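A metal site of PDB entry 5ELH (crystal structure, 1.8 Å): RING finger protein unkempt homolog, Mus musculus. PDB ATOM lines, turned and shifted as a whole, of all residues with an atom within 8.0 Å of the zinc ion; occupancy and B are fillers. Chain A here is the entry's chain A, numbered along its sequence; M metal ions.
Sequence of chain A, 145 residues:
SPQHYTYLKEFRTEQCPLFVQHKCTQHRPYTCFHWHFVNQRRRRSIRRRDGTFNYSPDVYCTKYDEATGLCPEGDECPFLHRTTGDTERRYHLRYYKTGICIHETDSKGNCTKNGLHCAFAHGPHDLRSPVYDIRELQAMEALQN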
ATOM      1  N   ARG A  43     -18.982  14.922  10.260  1.00  0.00           N
ATOM      2  CA  ARG A  43     -17.793  15.083  11.075  1.00  0.00           C
ATOM      3  C   ARG A  43     -16.623  14.371  10.404  1.00  0.00           C
ATOM      4  O   ARG A  43     -16.752  13.236   9.950  1.00  0.00           O
ATOM      5  CB  ARG A  43     -17.984  14.434  12.445  1.00  0.00           C
ATOM      6  CG  ARG A  43     -19.142  14.971  13.259  1.00  0.00           C
ATOM      7  CD  ARG A  43     -19.377  14.080  14.455  1.00  0.00           C
ATOM      8  NE  ARG A  43     -19.904  12.771  14.069  1.00  0.00           N
ATOM      9  CZ  ARG A  43     -19.913  11.697  14.855  1.00  0.00           C
ATOM     10  NH1 ARG A  43     -19.411  11.764  16.087  1.00  0.00           N
ATOM     11  NH2 ARG A  43     -20.425  10.558  14.418  1.00  0.00           N
ATOM     12  N   TYR A  55     -14.989   8.071  15.857  1.00  0.00           N
ATOM     13  CA  TYR A  55     -16.251   7.350  15.764  1.00  0.00           C
ATOM     14  C   TYR A  55     -16.181   6.177  14.791  1.00  0.00           C
ATOM     15  O   TYR A  55     -15.397   6.196  13.835  1.00  0.00           O
ATOM     16  CB  TYR A  55     -17.401   8.287  15.386  1.00  0.00           C
ATOM     17  CG  TYR A  55     -17.317   8.930  14.010  1.00  0.00           C
ATOM     18  CD1 TYR A  55     -17.819   8.296  12.899  1.00  0.00           C
ATOM     19  CD2 TYR A  55     -16.778  10.205  13.838  1.00  0.00           C
ATOM     20  CE1 TYR A  55     -17.771   8.884  11.640  1.00  0.00           C
ATOM     21  CE2 TYR A  55     -16.714  10.803  12.602  1.00  0.00           C
ATOM     22  CZ  TYR A  55     -17.209  10.135  11.500  1.00  0.00           C
ATOM     23  OH  TYR A  55     -17.150  10.724  10.253  1.00  0.00           O
ATOM     24  N   VAL A  59     -20.830   0.913  13.326  1.00  0.00           N
ATOM     25  CA  VAL A  59     -21.972   0.870  14.236  1.00  0.00           C
ATOM     26  C   VAL A  59     -22.661   2.251  14.344  1.00  0.00           C
ATOM     27  O   VAL A  59     -22.063   3.236  14.781  1.00  0.00           O
ATOM     28  CB  VAL A  59     -21.634   0.220  15.618  1.00  0.00           C
ATOM     29  CG1 VAL A  59     -20.140   0.009  15.796  1.00  0.00           C
ATOM     30  CG2 VAL A  59     -22.238   1.007  16.780  1.00  0.00           C
ATOM     31  N   TYR A  60     -23.903   2.288  13.887  1.00  0.00           N
ATOM     32  CA  TYR A  60     -24.655   3.534  13.774  1.00  0.00           C
ATOM     33  C   TYR A  60     -25.217   4.004  15.124  1.00  0.00           C
ATOM     34  O   TYR A  60     -25.754   3.221  15.915  1.00  0.00           O
ATOM     35  CB  TYR A  60     -25.804   3.372  12.770  1.00  0.00           C
ATOM     36  CG  TYR A  60     -25.389   3.446  11.307  1.00  0.00           C
ATOM     37  CD1 TYR A  60     -25.242   4.683  10.673  1.00  0.00           C
ATOM     38  CD2 TYR A  60     -25.147   2.301  10.574  1.00  0.00           C
ATOM     39  CE1 TYR A  60     -24.865   4.758   9.326  1.00  0.00           C
ATOM     40  CE2 TYR A  60     -24.770   2.362   9.230  1.00  0.00           C
ATOM     41  CZ  TYR A  60     -24.635   3.595   8.614  1.00  0.00           C
ATOM     42  OH  TYR A  60     -24.256   3.653   7.292  1.00  0.00           O
ATOM     43  N   CYS A  61     -25.084   5.300  15.368  1.00  0.00           N
ATOM     44  CA  CYS A  61     -25.700   5.975  16.506  1.00  0.00           C
ATOM     45  C   CYS A  61     -27.219   5.869  16.436  1.00  0.00           C
ATOM     46  O   CYS A  61     -27.797   6.187  15.403  1.00  0.00           O
ATOM     47  CB  CYS A  61     -25.300   7.449  16.459  1.00  0.00           C
ATOM     48  SG  CYS A  61     -25.858   8.516  17.809  1.00  0.00           S
ATOM     49  N   THR A  62     -27.864   5.455  17.527  1.00  0.00           N
ATOM     50  CA  THR A  62     -29.332   5.432  17.559  1.00  0.00           C
ATOM     51  C   THR A  62     -29.948   6.745  18.078  1.00  0.00           C
ATOM     52  O   THR A  62     -31.159   6.942  17.966  1.00  0.00           O
ATOM     53  CB  THR A  62     -29.866   4.268  18.384  1.00  0.00           C
ATOM     54  OG1 THR A  62     -29.304   4.313  19.699  1.00  0.00           O
ATOM     55  CG2 THR A  62     -29.509   2.936  17.738  1.00  0.00           C
ATOM     56  N   LYS A  63     -29.134   7.639  18.620  1.00  0.00           N
ATOM     57  CA  LYS A  63     -29.619   8.922  19.147  1.00  0.00           C
ATOM     58  C   LYS A  63     -29.662  10.034  18.099  1.00  0.00           C
ATOM     59  O   LYS A  63     -30.387  11.013  18.255  1.00  0.00           O
ATOM     60  CB  LYS A  63     -28.738   9.392  20.305  1.00  0.00           C
ATOM     61  CG  LYS A  63     -28.696   8.428  21.483  1.00  0.00           C
ATOM     62  CD  LYS A  63     -27.698   8.901  22.523  1.00  0.00           C
ATOM     63  CE  LYS A  63     -27.582   7.922  23.670  1.00  0.00           C
ATOM     64  NZ  LYS A  63     -26.430   8.242  24.559  1.00  0.00           N
ATOM     65  N   TYR A  64     -28.881   9.880  17.028  1.00  0.00           N
ATOM     66  CA  TYR A  64     -28.776  10.889  15.985  1.00  0.00           C
ATOM     67  C   TYR A  64     -30.135  11.109  15.304  1.00  0.00           C
ATOM     68  O   TYR A  64     -30.715  10.183  14.766  1.00  0.00           O
ATOM     69  CB  TYR A  64     -27.732  10.461  14.942  1.00  0.00           C
ATOM     70  CG  TYR A  64     -27.568  11.433  13.786  1.00  0.00           C
ATOM     71  CD1 TYR A  64     -26.878  12.625  13.953  1.00  0.00           C
ATOM     72  CD2 TYR A  64     -28.086  11.146  12.529  1.00  0.00           C
ATOM     73  CE1 TYR A  64     -26.718  13.510  12.907  1.00  0.00           C
ATOM     74  CE2 TYR A  64     -27.926  12.017  11.485  1.00  0.00           C
ATOM     75  CZ  TYR A  64     -27.233  13.190  11.668  1.00  0.00           C
ATOM     76  OH  TYR A  64     -27.072  14.075  10.622  1.00  0.00           O
ATOM     77  N   ASP A  65     -30.625  12.340  15.368  1.00  0.00           N
ATOM     78  CA  ASP A  65     -31.874  12.705  14.698  1.00  0.00           C
ATOM     79  C   ASP A  65     -31.588  13.071  13.249  1.00  0.00           C
ATOM     80  O   ASP A  65     -31.025  14.132  12.978  1.00  0.00           O
ATOM     81  CB  ASP A  65     -32.558  13.863  15.418  1.00  0.00           C
ATOM     82  CG  ASP A  65     -33.961  14.145  14.903  1.00  0.00           C
ATOM     83  OD1 ASP A  65     -34.318  13.663  13.811  1.00  0.00           O
ATOM     84  OD2 ASP A  65     -34.714  14.854  15.599  1.00  0.00           O
ATOM     85  N   LEU A  70     -28.960  16.528  14.541  1.00  0.00           N
ATOM     86  CA  LEU A  70     -28.453  16.707  15.911  1.00  0.00           C
ATOM     87  C   LEU A  70     -28.285  15.393  16.664  1.00  0.00           C
ATOM     88  O   LEU A  70     -29.207  14.570  16.710  1.00  0.00           O
ATOM     89  CB  LEU A  70     -29.409  17.609  16.695  1.00  0.00           C
ATOM     90  CG  LEU A  70     -29.678  19.011  16.130  1.00  0.00           C
ATOM     91  CD1 LEU A  70     -30.689  19.738  17.008  1.00  0.00           C
ATOM     92  CD2 LEU A  70     -28.387  19.800  16.017  1.00  0.00           C
ATOM     93  N   CYS A  71     -27.110  15.203  17.259  1.00  0.00           N
ATOM     94  CA  CYS A  71     -26.872  14.115  18.228  1.00  0.00           C
ATOM     95  C   CYS A  71     -26.444  14.767  19.537  1.00  0.00           C
ATOM     96  O   CYS A  71     -25.554  15.619  19.529  1.00  0.00           O
ATOM     97  CB  CYS A  71     -25.745  13.194  17.776  1.00  0.00           C
ATOM     98  SG  CYS A  71     -25.233  12.002  19.057  1.00  0.00           S
ATOM     99  N   PRO A  72     -27.062  14.367  20.664  1.00  0.00           N
ATOM    100  CA  PRO A  72     -26.698  14.985  21.942  1.00  0.00           C
ATOM    101  C   PRO A  72     -25.190  14.976  22.241  1.00  0.00           C
ATOM    102  O   PRO A  72     -24.735  15.861  22.965  1.00  0.00           O
ATOM    103  CB  PRO A  72     -27.431  14.129  22.970  1.00  0.00           C
ATOM    104  CG  PRO A  72     -28.555  13.522  22.238  1.00  0.00           C
ATOM    105  CD  PRO A  72     -28.098  13.326  20.839  1.00  0.00           C
ATOM    106  N   GLU A  73     -24.428  14.026  21.711  1.00  0.00           N
ATOM    107  CA  GLU A  73     -22.990  13.960  22.003  1.00  0.00           C
ATOM    108  C   GLU A  73     -22.127  14.730  20.994  1.00  0.00           C
ATOM    109  O   GLU A  73     -20.931  14.920  21.206  1.00  0.00           O
ATOM    110  CB  GLU A  73     -22.504  12.514  22.097  1.00  0.00           C
ATOM    111  CG  GLU A  73     -22.404  11.968  23.513  1.00  0.00           C
ATOM    112  CD  GLU A  73     -23.743  11.521  24.093  1.00  0.00           C
ATOM    113  OE1 GLU A  73     -24.627  11.102  23.313  1.00  0.00           O
ATOM    114  OE2 GLU A  73     -23.900  11.587  25.332  1.00  0.00           O
ATOM    115  N   GLY A  74     -22.746  15.175  19.905  1.00  0.00           N
ATOM    116  CA  GLY A  74     -22.053  15.971  18.899  1.00  0.00           C
ATOM    117  C   GLY A  74     -20.796  15.306  18.368  1.00  0.00           C
ATOM    118  O   GLY A  74     -20.790  14.098  18.111  1.00  0.00           O
ATOM    119  N   ASP A  75     -19.719  16.080  18.234  1.00  0.00           N
ATOM    120  CA  ASP A  75     -18.475  15.583  17.677  1.00  0.00           C
ATOM    121  C   ASP A  75     -17.843  14.481  18.531  1.00  0.00           C
ATOM    122  O   ASP A  75     -16.982  13.752  18.045  1.00  0.00           O
ATOM    123  CB  ASP A  75     -17.464  16.733  17.505  1.00  0.00           C
ATOM    124  CG  ASP A  75     -17.817  17.664  16.348  1.00  0.00           C
ATOM    125  OD1 ASP A  75     -18.795  17.389  15.632  1.00  0.00           O
ATOM    126  OD2 ASP A  75     -17.105  18.673  16.158  1.00  0.00           O
ATOM    127  N   GLU A  76     -18.269  14.347  19.792  1.00  0.00           N
ATOM    128  CA  GLU A  76     -17.673  13.375  20.684  1.00  0.00           C
ATOM    129  C   GLU A  76     -18.410  12.036  20.722  1.00  0.00           C
ATOM    130  O   GLU A  76     -18.008  11.125  21.457  1.00  0.00           O
ATOM    131  CB  GLU A  76     -17.555  13.946  22.107  1.00  0.00           C
ATOM    132  CG  GLU A  76     -16.646  15.166  22.179  1.00  0.00           C
ATOM    133  CD  GLU A  76     -15.288  14.914  21.520  1.00  0.00           C
ATOM    134  OE1 GLU A  76     -14.650  13.892  21.854  1.00  0.00           O
ATOM    135  OE2 GLU A  76     -14.880  15.728  20.657  1.00  0.00           O
ATOM    136  N   CYS A  77     -19.462  11.907  19.937  1.00  0.00           N
ATOM    137  CA  CYS A  77     -20.190  10.651  19.846  1.00  0.00           C
ATOM    138  C   CYS A  77     -19.307   9.618  19.163  1.00  0.00           C
ATOM    139  O   CYS A  77     -18.802   9.875  18.066  1.00  0.00           O
ATOM    140  CB  CYS A  77     -21.471  10.817  19.038  1.00  0.00           C
ATOM    141  SG  CYS A  77     -22.465   9.329  18.985  1.00  0.00           S
ATOM    142  N   PRO A  78     -19.128   8.440  19.797  1.00  0.00           N
ATOM    143  CA  PRO A  78     -18.249   7.420  19.216  1.00  0.00           C
ATOM    144  C   PRO A  78     -18.909   6.560  18.150  1.00  0.00           C
ATOM    145  O   PRO A  78     -18.279   5.610  17.648  1.00  0.00           O
ATOM    146  CB  PRO A  78     -17.878   6.552  20.407  1.00  0.00           C
ATOM    147  CG  PRO A  78     -19.060   6.646  21.312  1.00  0.00           C
ATOM    148  CD  PRO A  78     -19.629   8.040  21.122  1.00  0.00           C
ATOM    149  N   PHE A  79     -20.152   6.871  17.807  1.00  0.00           N
ATOM    150  CA  PHE A  79     -20.902   6.095  16.828  1.00  0.00           C
ATOM    151  C   PHE A  79     -21.151   6.876  15.537  1.00  0.00           C
ATOM    152  O   PHE A  79     -21.028   8.103  15.488  1.00  0.00           O
ATOM    153  CB  PHE A  79     -22.223   5.629  17.426  1.00  0.00           C
ATOM    154  CG  PHE A  79     -22.063   4.879  18.719  1.00  0.00           C
ATOM    155  CD1 PHE A  79     -21.417   3.657  18.758  1.00  0.00           C
ATOM    156  CD2 PHE A  79     -22.547   5.408  19.899  1.00  0.00           C
ATOM    157  CE1 PHE A  79     -21.261   2.972  19.942  1.00  0.00           C
ATOM    158  CE2 PHE A  79     -22.405   4.723  21.079  1.00  0.00           C
ATOM    159  CZ  PHE A  79     -21.763   3.506  21.106  1.00  0.00           C
ATOM    160  N   LEU A  80     -21.511   6.127  14.517  1.00  0.00           N
ATOM    161  CA  LEU A  80     -21.680   6.652  13.172  1.00  0.00           C
ATOM    162  C   LEU A  80     -23.041   7.307  12.994  1.00  0.00           C
ATOM    163  O   LEU A  80     -24.059   6.778  13.442  1.00  0.00           O
ATOM    164  CB  LEU A  80     -21.525   5.480  12.211  1.00  0.00           C
ATOM    165  CG  LEU A  80     -21.594   5.774  10.726  1.00  0.00           C
ATOM    166  CD1 LEU A  80     -20.485   6.717  10.305  1.00  0.00           C
ATOM    167  CD2 LEU A  80     -21.506   4.444   9.989  1.00  0.00           C
ATOM    168  N   HIS A  81     -23.064   8.473  12.350  1.00  0.00           N
ATOM    169  CA  HIS A  81     -24.314   9.180  12.076  1.00  0.00           C
ATOM    170  C   HIS A  81     -24.724   8.993  10.638  1.00  0.00           C
ATOM    171  O   HIS A  81     -23.919   9.128   9.728  1.00  0.00           O
ATOM    172  CB  HIS A  81     -24.147  10.663  12.397  1.00  0.00           C
ATOM    173  CG  HIS A  81     -23.907  10.916  13.862  1.00  0.00           C
ATOM    174  ND1 HIS A  81     -23.386  12.099  14.345  1.00  0.00           N
ATOM    175  CD2 HIS A  81     -24.108  10.125  14.942  1.00  0.00           C
ATOM    176  CE1 HIS A  81     -23.294  12.030  15.655  1.00  0.00           C
ATOM    177  NE2 HIS A  81     -23.718  10.839  16.050  1.00  0.00           N
ATOM    178  N   ARG A  82     -25.996   8.666  10.455  1.00  0.00           N
ATOM    179  CA  ARG A  82     -26.550   8.475   9.128  1.00  0.00           C
ATOM    180  C   ARG A  82     -26.939   9.841   8.550  1.00  0.00           C
ATOM    181  O   ARG A  82     -28.103  10.198   8.492  1.00  0.00           O
ATOM    182  CB  ARG A  82     -27.752   7.533   9.168  1.00  0.00           C
ATOM    183  CG  ARG A  82     -27.962   6.766   7.875  1.00  0.00           C
ATOM    184  CD  ARG A  82     -29.185   5.870   7.962  1.00  0.00           C
ATOM    185  NE  ARG A  82     -29.171   4.990   9.127  1.00  0.00           N
ATOM    186  CZ  ARG A  82     -28.630   3.774   9.148  1.00  0.00           C
ATOM    187  NH1 ARG A  82     -28.042   3.277   8.073  1.00  0.00           N
ATOM    188  NH2 ARG A  82     -28.682   3.059  10.263  1.00  0.00           N
ATOM    189  N   GLU A  88     -20.880  10.204   6.386  1.00  0.00           N
ATOM    190  CA  GLU A  88     -19.871   9.955   7.413  1.00  0.00           C
ATOM    191  C   GLU A  88     -19.174   8.618   7.151  1.00  0.00           C
ATOM    192  O   GLU A  88     -17.971   8.494   7.341  1.00  0.00           O
ATOM    193  CB  GLU A  88     -20.455  10.022   8.836  1.00  0.00           C
ATOM    194  CG  GLU A  88     -20.630  11.451   9.331  1.00  0.00           C
ATOM    195  CD  GLU A  88     -20.756  11.569  10.843  1.00  0.00           C
ATOM    196  OE1 GLU A  88     -20.881  10.530  11.539  1.00  0.00           O
ATOM    197  OE2 GLU A  88     -20.703  12.706  11.339  1.00  0.00           O
HETATM  198 ZN    ZN M   1     -24.336  10.158  17.895  1.00  0.00          ZN
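Within 4 Å of the zinc ion: Cys 61, Cys 71, Cys 77 and His 81.
The zinc ion is bound by NE2 of His 81 (2.1 Å), SG of Cys 61 (2.2 Å), SG of Cys 77 (2.3 Å) and SG of Cys 71 (2.4 Å).
The zinc ion has four donor atoms within binding distance.
A ring nitrogen (ND1) of His 81 lies within hydrogen-bond range of the guanidinium group (NH2) of Arg 43, 3.3 Å away.
The side-chain carboxylate of Glu 88 lies within hydrogen-bond range of the backbone NH of His 81 (3.1 Å).
The side-chain sulfur (SG) of Cys 61 sits close to the backbone NH (N) of Tyr 64 (3.4 Å).
The backbone NH (N) of Lys 63 lies close to the side-chain sulfur (SG) of Cys 61 (3.5 Å).
The backbone NH (N) of Cys 61 lies within hydrogen-bond range of the backbone carbonyl oxygen (O) of Leu 80 (2.6 Å).
SG of Cys 77 sits close to N of Phe 79, 3.6 Å away.
O of Cys 77 is in hydrogen-bond range of NH1 of Arg 43, at 2.8 Å.
SG of Cys 71 lies close to N of Glu 73 (3.4 Å).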
